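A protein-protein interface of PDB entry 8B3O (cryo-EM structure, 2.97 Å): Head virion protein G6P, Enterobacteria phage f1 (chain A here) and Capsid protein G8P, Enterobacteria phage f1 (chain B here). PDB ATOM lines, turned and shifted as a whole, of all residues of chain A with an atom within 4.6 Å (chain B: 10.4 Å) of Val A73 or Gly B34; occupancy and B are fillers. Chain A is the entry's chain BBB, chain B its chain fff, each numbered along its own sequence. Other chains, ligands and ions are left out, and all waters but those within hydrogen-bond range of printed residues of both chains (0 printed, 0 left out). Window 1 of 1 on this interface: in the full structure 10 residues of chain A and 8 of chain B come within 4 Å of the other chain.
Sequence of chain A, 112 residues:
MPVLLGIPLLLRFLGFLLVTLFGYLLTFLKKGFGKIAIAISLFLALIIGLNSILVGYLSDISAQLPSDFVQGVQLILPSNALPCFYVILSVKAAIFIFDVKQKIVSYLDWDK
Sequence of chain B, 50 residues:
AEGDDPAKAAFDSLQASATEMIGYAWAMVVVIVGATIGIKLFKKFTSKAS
Hydrophobic or aromatic side chains of chain A that line the printed part of chain B: Phe A69, Val A73, Ile A76 and Leu A77.
Hydrophobic or aromatic side chains of chain B that line the printed part of chain A: Val B31, Val B33, Ala B35, Ile B39 and Phe B42.
Among the printed residues, no Asp or Glu carboxylate lies within 4 Å of a Lys or Arg side-chain nitrogen of the other chain.
Among the printed residues, merely in contact across the chains: Ile A76 with Ala B35, Gly A72 with Val B31, Ile A76 with Ile B39, Phe A69 with Val B33, Leu A77 with Phe B42, Gln A71 with Val B31, Phe A69 with Gly B34, Gly A72 with Ala B35 and Val A73 with Gly B34.
Printed residues of chain B within 4 Å of Phe A69: Val B33 (3.6 Å) and Gly B34 (3.8 Å).
Val A70 touches none of the printed residues of chain B.
Of the printed residues of chain B, Gln A71 touches Val B31.
Gln A74 touches none of the printed residues of chain B.
Of chain B, only Ala B35 and Ile B39 come within 4 Å of Ile A76.
Val B30 touches none of the printed residues of chain A.
Of the printed residues of chain A, Val B33 touches Phe A69 (3.6 Å).
Of the printed residues of chain A, Ala B35 touches Gly A72 (3.9 Å) and Ile A76 (3.3 Å).
Of the printed residues of chain A, Phe B42 touches Leu A77.
The nearest printed residue of chain B that does not touch Val A73 is Ala B35 (4.4 Å).
The nearest printed residue of chain A that does not touch Gly B34 is Gly A72 (4.3 Å).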
ATOM      1  N   PHE A  69     -11.357  28.078  17.572  1.00  0.00           N
ATOM      2  CA  PHE A  69     -12.233  26.944  17.321  1.00  0.00           C
ATOM      3  C   PHE A  69     -11.422  25.737  16.865  1.00  0.00           C
ATOM      4  O   PHE A  69     -11.911  24.933  16.073  1.00  0.00           O
ATOM      5  CB  PHE A  69     -13.281  27.285  16.259  1.00  0.00           C
ATOM      6  CG  PHE A  69     -14.353  28.233  16.726  1.00  0.00           C
ATOM      7  CD1 PHE A  69     -15.475  27.768  17.398  1.00  0.00           C
ATOM      8  CD2 PHE A  69     -14.225  29.595  16.508  1.00  0.00           C
ATOM      9  CE1 PHE A  69     -16.452  28.653  17.835  1.00  0.00           C
ATOM     10  CE2 PHE A  69     -15.199  30.477  16.945  1.00  0.00           C
ATOM     11  CZ  PHE A  69     -16.310  30.005  17.608  1.00  0.00           C
ATOM     12  N   VAL A  70     -10.185  25.626  17.364  1.00  0.00           N
ATOM     13  CA  VAL A  70      -9.328  24.491  17.055  1.00  0.00           C
ATOM     14  C   VAL A  70      -9.368  23.506  18.221  1.00  0.00           C
ATOM     15  O   VAL A  70      -9.614  22.320  18.010  1.00  0.00           O
ATOM     16  CB  VAL A  70      -7.896  24.921  16.673  1.00  0.00           C
ATOM     17  CG1 VAL A  70      -6.894  23.779  16.780  1.00  0.00           C
ATOM     18  CG2 VAL A  70      -7.847  25.528  15.278  1.00  0.00           C
ATOM     19  N   GLN A  71      -9.156  24.016  19.443  1.00  0.00           N
ATOM     20  CA  GLN A  71      -9.143  23.205  20.652  1.00  0.00           C
ATOM     21  C   GLN A  71     -10.358  22.278  20.689  1.00  0.00           C
ATOM     22  O   GLN A  71     -10.267  21.173  21.216  1.00  0.00           O
ATOM     23  CB  GLN A  71      -9.075  24.083  21.904  1.00  0.00           C
ATOM     24  CG  GLN A  71      -8.589  23.331  23.139  1.00  0.00           C
ATOM     25  CD  GLN A  71      -8.798  24.056  24.449  1.00  0.00           C
ATOM     26  OE1 GLN A  71      -9.153  23.454  25.461  1.00  0.00           O
ATOM     27  NE2 GLN A  71      -8.566  25.360  24.449  1.00  0.00           N
ATOM     28  N   GLY A  72     -11.478  22.738  20.115  1.00  0.00           N
ATOM     29  CA  GLY A  72     -12.688  21.942  19.981  1.00  0.00           C
ATOM     30  C   GLY A  72     -12.494  20.767  19.026  1.00  0.00           C
ATOM     31  O   GLY A  72     -12.496  19.610  19.450  1.00  0.00           O
ATOM     32  N   VAL A  73     -12.284  21.086  17.743  1.00  0.00           N
ATOM     33  CA  VAL A  73     -12.210  20.087  16.685  1.00  0.00           C
ATOM     34  C   VAL A  73     -11.196  19.003  17.062  1.00  0.00           C
ATOM     35  O   VAL A  73     -11.423  17.833  16.773  1.00  0.00           O
ATOM     36  CB  VAL A  73     -11.935  20.703  15.297  1.00  0.00           C
ATOM     37  CG1 VAL A  73     -12.157  19.703  14.171  1.00  0.00           C
ATOM     38  CG2 VAL A  73     -12.779  21.945  15.047  1.00  0.00           C
ATOM     39  N   GLN A  74     -10.124  19.380  17.772  1.00  0.00           N
ATOM     40  CA  GLN A  74      -9.060  18.446  18.111  1.00  0.00           C
ATOM     41  C   GLN A  74      -9.325  17.776  19.459  1.00  0.00           C
ATOM     42  O   GLN A  74      -8.402  17.582  20.250  1.00  0.00           O
ATOM     43  CB  GLN A  74      -7.703  19.152  18.129  1.00  0.00           C
ATOM     44  CG  GLN A  74      -7.163  19.495  16.751  1.00  0.00           C
ATOM     45  CD  GLN A  74      -5.692  19.838  16.779  1.00  0.00           C
ATOM     46  OE1 GLN A  74      -5.174  20.393  17.747  1.00  0.00           O
ATOM     47  NE2 GLN A  74      -5.002  19.504  15.702  1.00  0.00           N
ATOM     48  N   LEU A  75     -10.585  17.406  19.707  1.00  0.00           N
ATOM     49  CA  LEU A  75     -10.984  16.720  20.926  1.00  0.00           C
ATOM     50  C   LEU A  75     -12.042  15.682  20.560  1.00  0.00           C
ATOM     51  O   LEU A  75     -12.392  14.816  21.360  1.00  0.00           O
ATOM     52  CB  LEU A  75     -11.521  17.772  21.906  1.00  0.00           C
ATOM     53  CG  LEU A  75     -11.780  17.325  23.345  1.00  0.00           C
ATOM     54  CD1 LEU A  75     -11.248  18.349  24.337  1.00  0.00           C
ATOM     55  CD2 LEU A  75     -13.265  17.090  23.574  1.00  0.00           C
ATOM     56  N   ILE A  76     -12.509  15.772  19.313  1.00  0.00           N
ATOM     57  CA  ILE A  76     -13.680  15.054  18.849  1.00  0.00           C
ATOM     58  C   ILE A  76     -13.307  14.239  17.612  1.00  0.00           C
ATOM     59  O   ILE A  76     -13.932  13.212  17.338  1.00  0.00           O
ATOM     60  CB  ILE A  76     -14.822  16.069  18.614  1.00  0.00           C
ATOM     61  CG1 ILE A  76     -15.226  16.774  19.915  1.00  0.00           C
ATOM     62  CG2 ILE A  76     -16.020  15.456  17.906  1.00  0.00           C
ATOM     63  CD1 ILE A  76     -15.621  15.848  21.052  1.00  0.00           C
ATOM     64  N   LEU A  77     -12.264  14.683  16.897  1.00  0.00           N
ATOM     65  CA  LEU A  77     -11.893  14.103  15.617  1.00  0.00           C
ATOM     66  C   LEU A  77     -11.300  12.709  15.816  1.00  0.00           C
ATOM     67  O   LEU A  77     -10.363  12.544  16.596  1.00  0.00           O
ATOM     68  CB  LEU A  77     -10.900  15.035  14.914  1.00  0.00           C
ATOM     69  CG  LEU A  77     -11.158  15.256  13.424  1.00  0.00           C
ATOM     70  CD1 LEU A  77     -12.605  15.661  13.184  1.00  0.00           C
ATOM     71  CD2 LEU A  77     -10.210  16.302  12.861  1.00  0.00           C
ATOM     72  N   TRP B  26     -16.910  31.831  29.204  1.00  0.00           N
ATOM     73  CA  TRP B  26     -16.687  32.195  27.811  1.00  0.00           C
ATOM     74  C   TRP B  26     -15.642  31.280  27.179  1.00  0.00           C
ATOM     75  O   TRP B  26     -15.639  31.114  25.967  1.00  0.00           O
ATOM     76  CB  TRP B  26     -16.339  33.678  27.632  1.00  0.00           C
ATOM     77  CG  TRP B  26     -17.525  34.550  27.347  1.00  0.00           C
ATOM     78  CD1 TRP B  26     -18.043  35.514  28.163  1.00  0.00           C
ATOM     79  CD2 TRP B  26     -18.357  34.542  26.170  1.00  0.00           C
ATOM     80  NE1 TRP B  26     -19.133  36.104  27.583  1.00  0.00           N
ATOM     81  CE2 TRP B  26     -19.350  35.531  26.359  1.00  0.00           C
ATOM     82  CE3 TRP B  26     -18.363  33.805  24.976  1.00  0.00           C
ATOM     83  CZ2 TRP B  26     -20.332  35.797  25.402  1.00  0.00           C
ATOM     84  CZ3 TRP B  26     -19.334  34.068  24.032  1.00  0.00           C
ATOM     85  CH2 TRP B  26     -20.305  35.049  24.245  1.00  0.00           C
ATOM     86  N   ALA B  27     -14.789  30.676  28.017  1.00  0.00           N
ATOM     87  CA  ALA B  27     -13.818  29.689  27.574  1.00  0.00           C
ATOM     88  C   ALA B  27     -14.504  28.379  27.181  1.00  0.00           C
ATOM     89  O   ALA B  27     -14.273  27.877  26.082  1.00  0.00           O
ATOM     90  CB  ALA B  27     -12.761  29.476  28.633  1.00  0.00           C
ATOM     91  N   MET B  28     -15.349  27.850  28.079  1.00  0.00           N
ATOM     92  CA  MET B  28     -15.943  26.526  27.953  1.00  0.00           C
ATOM     93  C   MET B  28     -16.843  26.450  26.718  1.00  0.00           C
ATOM     94  O   MET B  28     -16.904  25.411  26.068  1.00  0.00           O
ATOM     95  CB  MET B  28     -16.756  26.166  29.201  1.00  0.00           C
ATOM     96  CG  MET B  28     -17.011  24.683  29.375  1.00  0.00           C
ATOM     97  SD  MET B  28     -18.201  24.370  30.702  1.00  0.00           S
ATOM     98  CE  MET B  28     -18.216  22.579  30.714  1.00  0.00           C
ATOM     99  N   VAL B  29     -17.523  27.559  26.398  1.00  0.00           N
ATOM    100  CA  VAL B  29     -18.486  27.597  25.310  1.00  0.00           C
ATOM    101  C   VAL B  29     -17.779  27.523  23.952  1.00  0.00           C
ATOM    102  O   VAL B  29     -18.372  27.047  22.993  1.00  0.00           O
ATOM    103  CB  VAL B  29     -19.446  28.800  25.439  1.00  0.00           C
ATOM    104  CG1 VAL B  29     -18.876  30.083  24.854  1.00  0.00           C
ATOM    105  CG2 VAL B  29     -20.825  28.508  24.866  1.00  0.00           C
ATOM    106  N   VAL B  30     -16.517  27.970  23.874  1.00  0.00           N
ATOM    107  CA  VAL B  30     -15.797  27.993  22.605  1.00  0.00           C
ATOM    108  C   VAL B  30     -15.209  26.610  22.312  1.00  0.00           C
ATOM    109  O   VAL B  30     -14.922  26.289  21.158  1.00  0.00           O
ATOM    110  CB  VAL B  30     -14.727  29.107  22.553  1.00  0.00           C
ATOM    111  CG1 VAL B  30     -14.135  29.281  21.160  1.00  0.00           C
ATOM    112  CG2 VAL B  30     -15.272  30.438  23.042  1.00  0.00           C
ATOM    113  N   VAL B  31     -15.021  25.801  23.364  1.00  0.00           N
ATOM    114  CA  VAL B  31     -14.493  24.450  23.230  1.00  0.00           C
ATOM    115  C   VAL B  31     -15.611  23.526  22.745  1.00  0.00           C
ATOM    116  O   VAL B  31     -15.385  22.675  21.887  1.00  0.00           O
ATOM    117  CB  VAL B  31     -13.836  23.957  24.539  1.00  0.00           C
ATOM    118  CG1 VAL B  31     -13.409  22.497  24.471  1.00  0.00           C
ATOM    119  CG2 VAL B  31     -12.657  24.828  24.953  1.00  0.00           C
ATOM    120  N   ILE B  32     -16.821  23.729  23.283  1.00  0.00           N
ATOM    121  CA  ILE B  32     -17.981  22.902  22.988  1.00  0.00           C
ATOM    122  C   ILE B  32     -18.575  23.269  21.625  1.00  0.00           C
ATOM    123  O   ILE B  32     -18.935  22.371  20.871  1.00  0.00           O
ATOM    124  CB  ILE B  32     -19.006  22.932  24.145  1.00  0.00           C
ATOM    125  CG1 ILE B  32     -18.384  22.370  25.428  1.00  0.00           C
ATOM    126  CG2 ILE B  32     -20.289  22.197  23.771  1.00  0.00           C
ATOM    127  CD1 ILE B  32     -19.235  22.512  26.669  1.00  0.00           C
ATOM    128  N   VAL B  33     -18.679  24.568  21.306  1.00  0.00           N
ATOM    129  CA  VAL B  33     -19.217  24.996  20.018  1.00  0.00           C
ATOM    130  C   VAL B  33     -18.290  24.542  18.885  1.00  0.00           C
ATOM    131  O   VAL B  33     -18.766  24.136  17.828  1.00  0.00           O
ATOM    132  CB  VAL B  33     -19.559  26.503  19.983  1.00  0.00           C
ATOM    133  CG1 VAL B  33     -19.597  27.093  18.578  1.00  0.00           C
ATOM    134  CG2 VAL B  33     -20.872  26.794  20.699  1.00  0.00           C
ATOM    135  N   GLY B  34     -16.974  24.572  19.133  1.00  0.00           N
ATOM    136  CA  GLY B  34     -15.987  24.054  18.197  1.00  0.00           C
ATOM    137  C   GLY B  34     -16.296  22.613  17.799  1.00  0.00           C
ATOM    138  O   GLY B  34     -16.434  22.310  16.614  1.00  0.00           O
ATOM    139  N   ALA B  35     -16.454  21.755  18.815  1.00  0.00           N
ATOM    140  CA  ALA B  35     -16.726  20.335  18.657  1.00  0.00           C
ATOM    141  C   ALA B  35     -17.984  20.103  17.820  1.00  0.00           C
ATOM    142  O   ALA B  35     -17.961  19.285  16.907  1.00  0.00           O
ATOM    143  CB  ALA B  35     -16.837  19.688  20.014  1.00  0.00           C
ATOM    144  N   THR B  36     -19.060  20.842  18.128  1.00  0.00           N
ATOM    145  CA  THR B  36     -20.366  20.659  17.511  1.00  0.00           C
ATOM    146  C   THR B  36     -20.320  20.993  16.018  1.00  0.00           C
ATOM    147  O   THR B  36     -20.909  20.264  15.219  1.00  0.00           O
ATOM    148  CB  THR B  36     -21.457  21.428  18.269  1.00  0.00           C
ATOM    149  OG1 THR B  36     -21.241  21.248  19.669  1.00  0.00           O
ATOM    150  CG2 THR B  36     -22.853  20.954  17.930  1.00  0.00           C
ATOM    151  N   ILE B  37     -19.602  22.066  15.659  1.00  0.00           N
ATOM    152  CA  ILE B  37     -19.472  22.502  14.273  1.00  0.00           C
ATOM    153  C   ILE B  37     -18.592  21.520  13.498  1.00  0.00           C
ATOM    154  O   ILE B  37     -18.766  21.373  12.289  1.00  0.00           O
ATOM    155  CB  ILE B  37     -18.981  23.963  14.176  1.00  0.00           C
ATOM    156  CG1 ILE B  37     -20.062  24.942  14.631  1.00  0.00           C
ATOM    157  CG2 ILE B  37     -18.480  24.315  12.777  1.00  0.00           C
ATOM    158  CD1 ILE B  37     -19.587  26.377  14.659  1.00  0.00           C
ATOM    159  N   GLY B  38     -17.703  20.818  14.218  1.00  0.00           N
ATOM    160  CA  GLY B  38     -16.759  19.869  13.649  1.00  0.00           C
ATOM    161  C   GLY B  38     -17.377  18.501  13.359  1.00  0.00           C
ATOM    162  O   GLY B  38     -16.895  17.800  12.468  1.00  0.00           O
ATOM    163  N   ILE B  39     -18.413  18.125  14.129  1.00  0.00           N
ATOM    164  CA  ILE B  39     -19.152  16.890  13.895  1.00  0.00           C
ATOM    165  C   ILE B  39     -20.096  17.104  12.713  1.00  0.00           C
ATOM    166  O   ILE B  39     -20.341  16.184  11.936  1.00  0.00           O
ATOM    167  CB  ILE B  39     -19.914  16.402  15.150  1.00  0.00           C
ATOM    168  CG1 ILE B  39     -18.996  16.187  16.355  1.00  0.00           C
ATOM    169  CG2 ILE B  39     -20.724  15.144  14.851  1.00  0.00           C
ATOM    170  CD1 ILE B  39     -19.726  15.958  17.665  1.00  0.00           C
ATOM    171  N   LYS B  40     -20.613  18.331  12.586  1.00  0.00           N
ATOM    172  CA  LYS B  40     -21.621  18.639  11.588  1.00  0.00           C
ATOM    173  C   LYS B  40     -21.016  18.756  10.187  1.00  0.00           C
ATOM    174  O   LYS B  40     -21.682  18.391   9.226  1.00  0.00           O
ATOM    175  CB  LYS B  40     -22.532  19.776  12.061  1.00  0.00           C
ATOM    176  CG  LYS B  40     -23.430  19.370  13.227  1.00  0.00           C
ATOM    177  CD  LYS B  40     -24.612  20.279  13.560  1.00  0.00           C
ATOM    178  CE  LYS B  40     -24.341  21.770  13.600  1.00  0.00           C
ATOM    179  NZ  LYS B  40     -24.319  22.339  14.970  1.00  0.00           N
ATOM    180  N   LEU B  41     -19.759  19.218  10.084  1.00  0.00           N
ATOM    181  CA  LEU B  41     -19.058  19.281   8.807  1.00  0.00           C
ATOM    182  C   LEU B  41     -18.724  17.879   8.299  1.00  0.00           C
ATOM    183  O   LEU B  41     -19.033  17.547   7.153  1.00  0.00           O
ATOM    184  CB  LEU B  41     -17.795  20.140   8.942  1.00  0.00           C
ATOM    185  CG  LEU B  41     -17.884  21.553   8.363  1.00  0.00           C
ATOM    186  CD1 LEU B  41     -16.546  22.268   8.483  1.00  0.00           C
ATOM    187  CD2 LEU B  41     -18.342  21.525   6.912  1.00  0.00           C
ATOM    188  N   PHE B  42     -18.093  17.065   9.156  1.00  0.00           N
ATOM    189  CA  PHE B  42     -17.623  15.756   8.738  1.00  0.00           C
ATOM    190  C   PHE B  42     -18.774  14.863   8.280  1.00  0.00           C
ATOM    191  O   PHE B  42     -18.644  14.211   7.251  1.00  0.00           O
ATOM    192  CB  PHE B  42     -16.620  15.165   9.730  1.00  0.00           C
ATOM    193  CG  PHE B  42     -15.214  15.633   9.461  1.00  0.00           C
ATOM    194  CD1 PHE B  42     -14.471  15.083   8.424  1.00  0.00           C
ATOM    195  CD2 PHE B  42     -14.645  16.654  10.210  1.00  0.00           C
ATOM    196  CE1 PHE B  42     -13.179  15.519   8.163  1.00  0.00           C
ATOM    197  CE2 PHE B  42     -13.355  17.095   9.946  1.00  0.00           C
ATOM    198  CZ  PHE B  42     -12.623  16.526   8.924  1.00  0.00           C
ATOM    199  N   PHE B  45     -19.889  16.012   4.611  1.00  0.00           N
ATOM    200  CA  PHE B  45     -18.936  15.569   3.602  1.00  0.00           C
ATOM    201  C   PHE B  45     -19.142  14.100   3.230  1.00  0.00           C
ATOM    202  O   PHE B  45     -18.705  13.667   2.169  1.00  0.00           O
ATOM    203  CB  PHE B  45     -17.493  15.697   4.100  1.00  0.00           C
ATOM    204  CG  PHE B  45     -16.945  17.091   4.269  1.00  0.00           C
ATOM    205  CD1 PHE B  45     -17.305  18.125   3.414  1.00  0.00           C
ATOM    206  CD2 PHE B  45     -16.015  17.352   5.266  1.00  0.00           C
ATOM    207  CE1 PHE B  45     -16.775  19.399   3.577  1.00  0.00           C
ATOM    208  CE2 PHE B  45     -15.486  18.625   5.429  1.00  0.00           C
ATOM    209  CZ  PHE B  45     -15.865  19.645   4.583  1.00  0.00           C
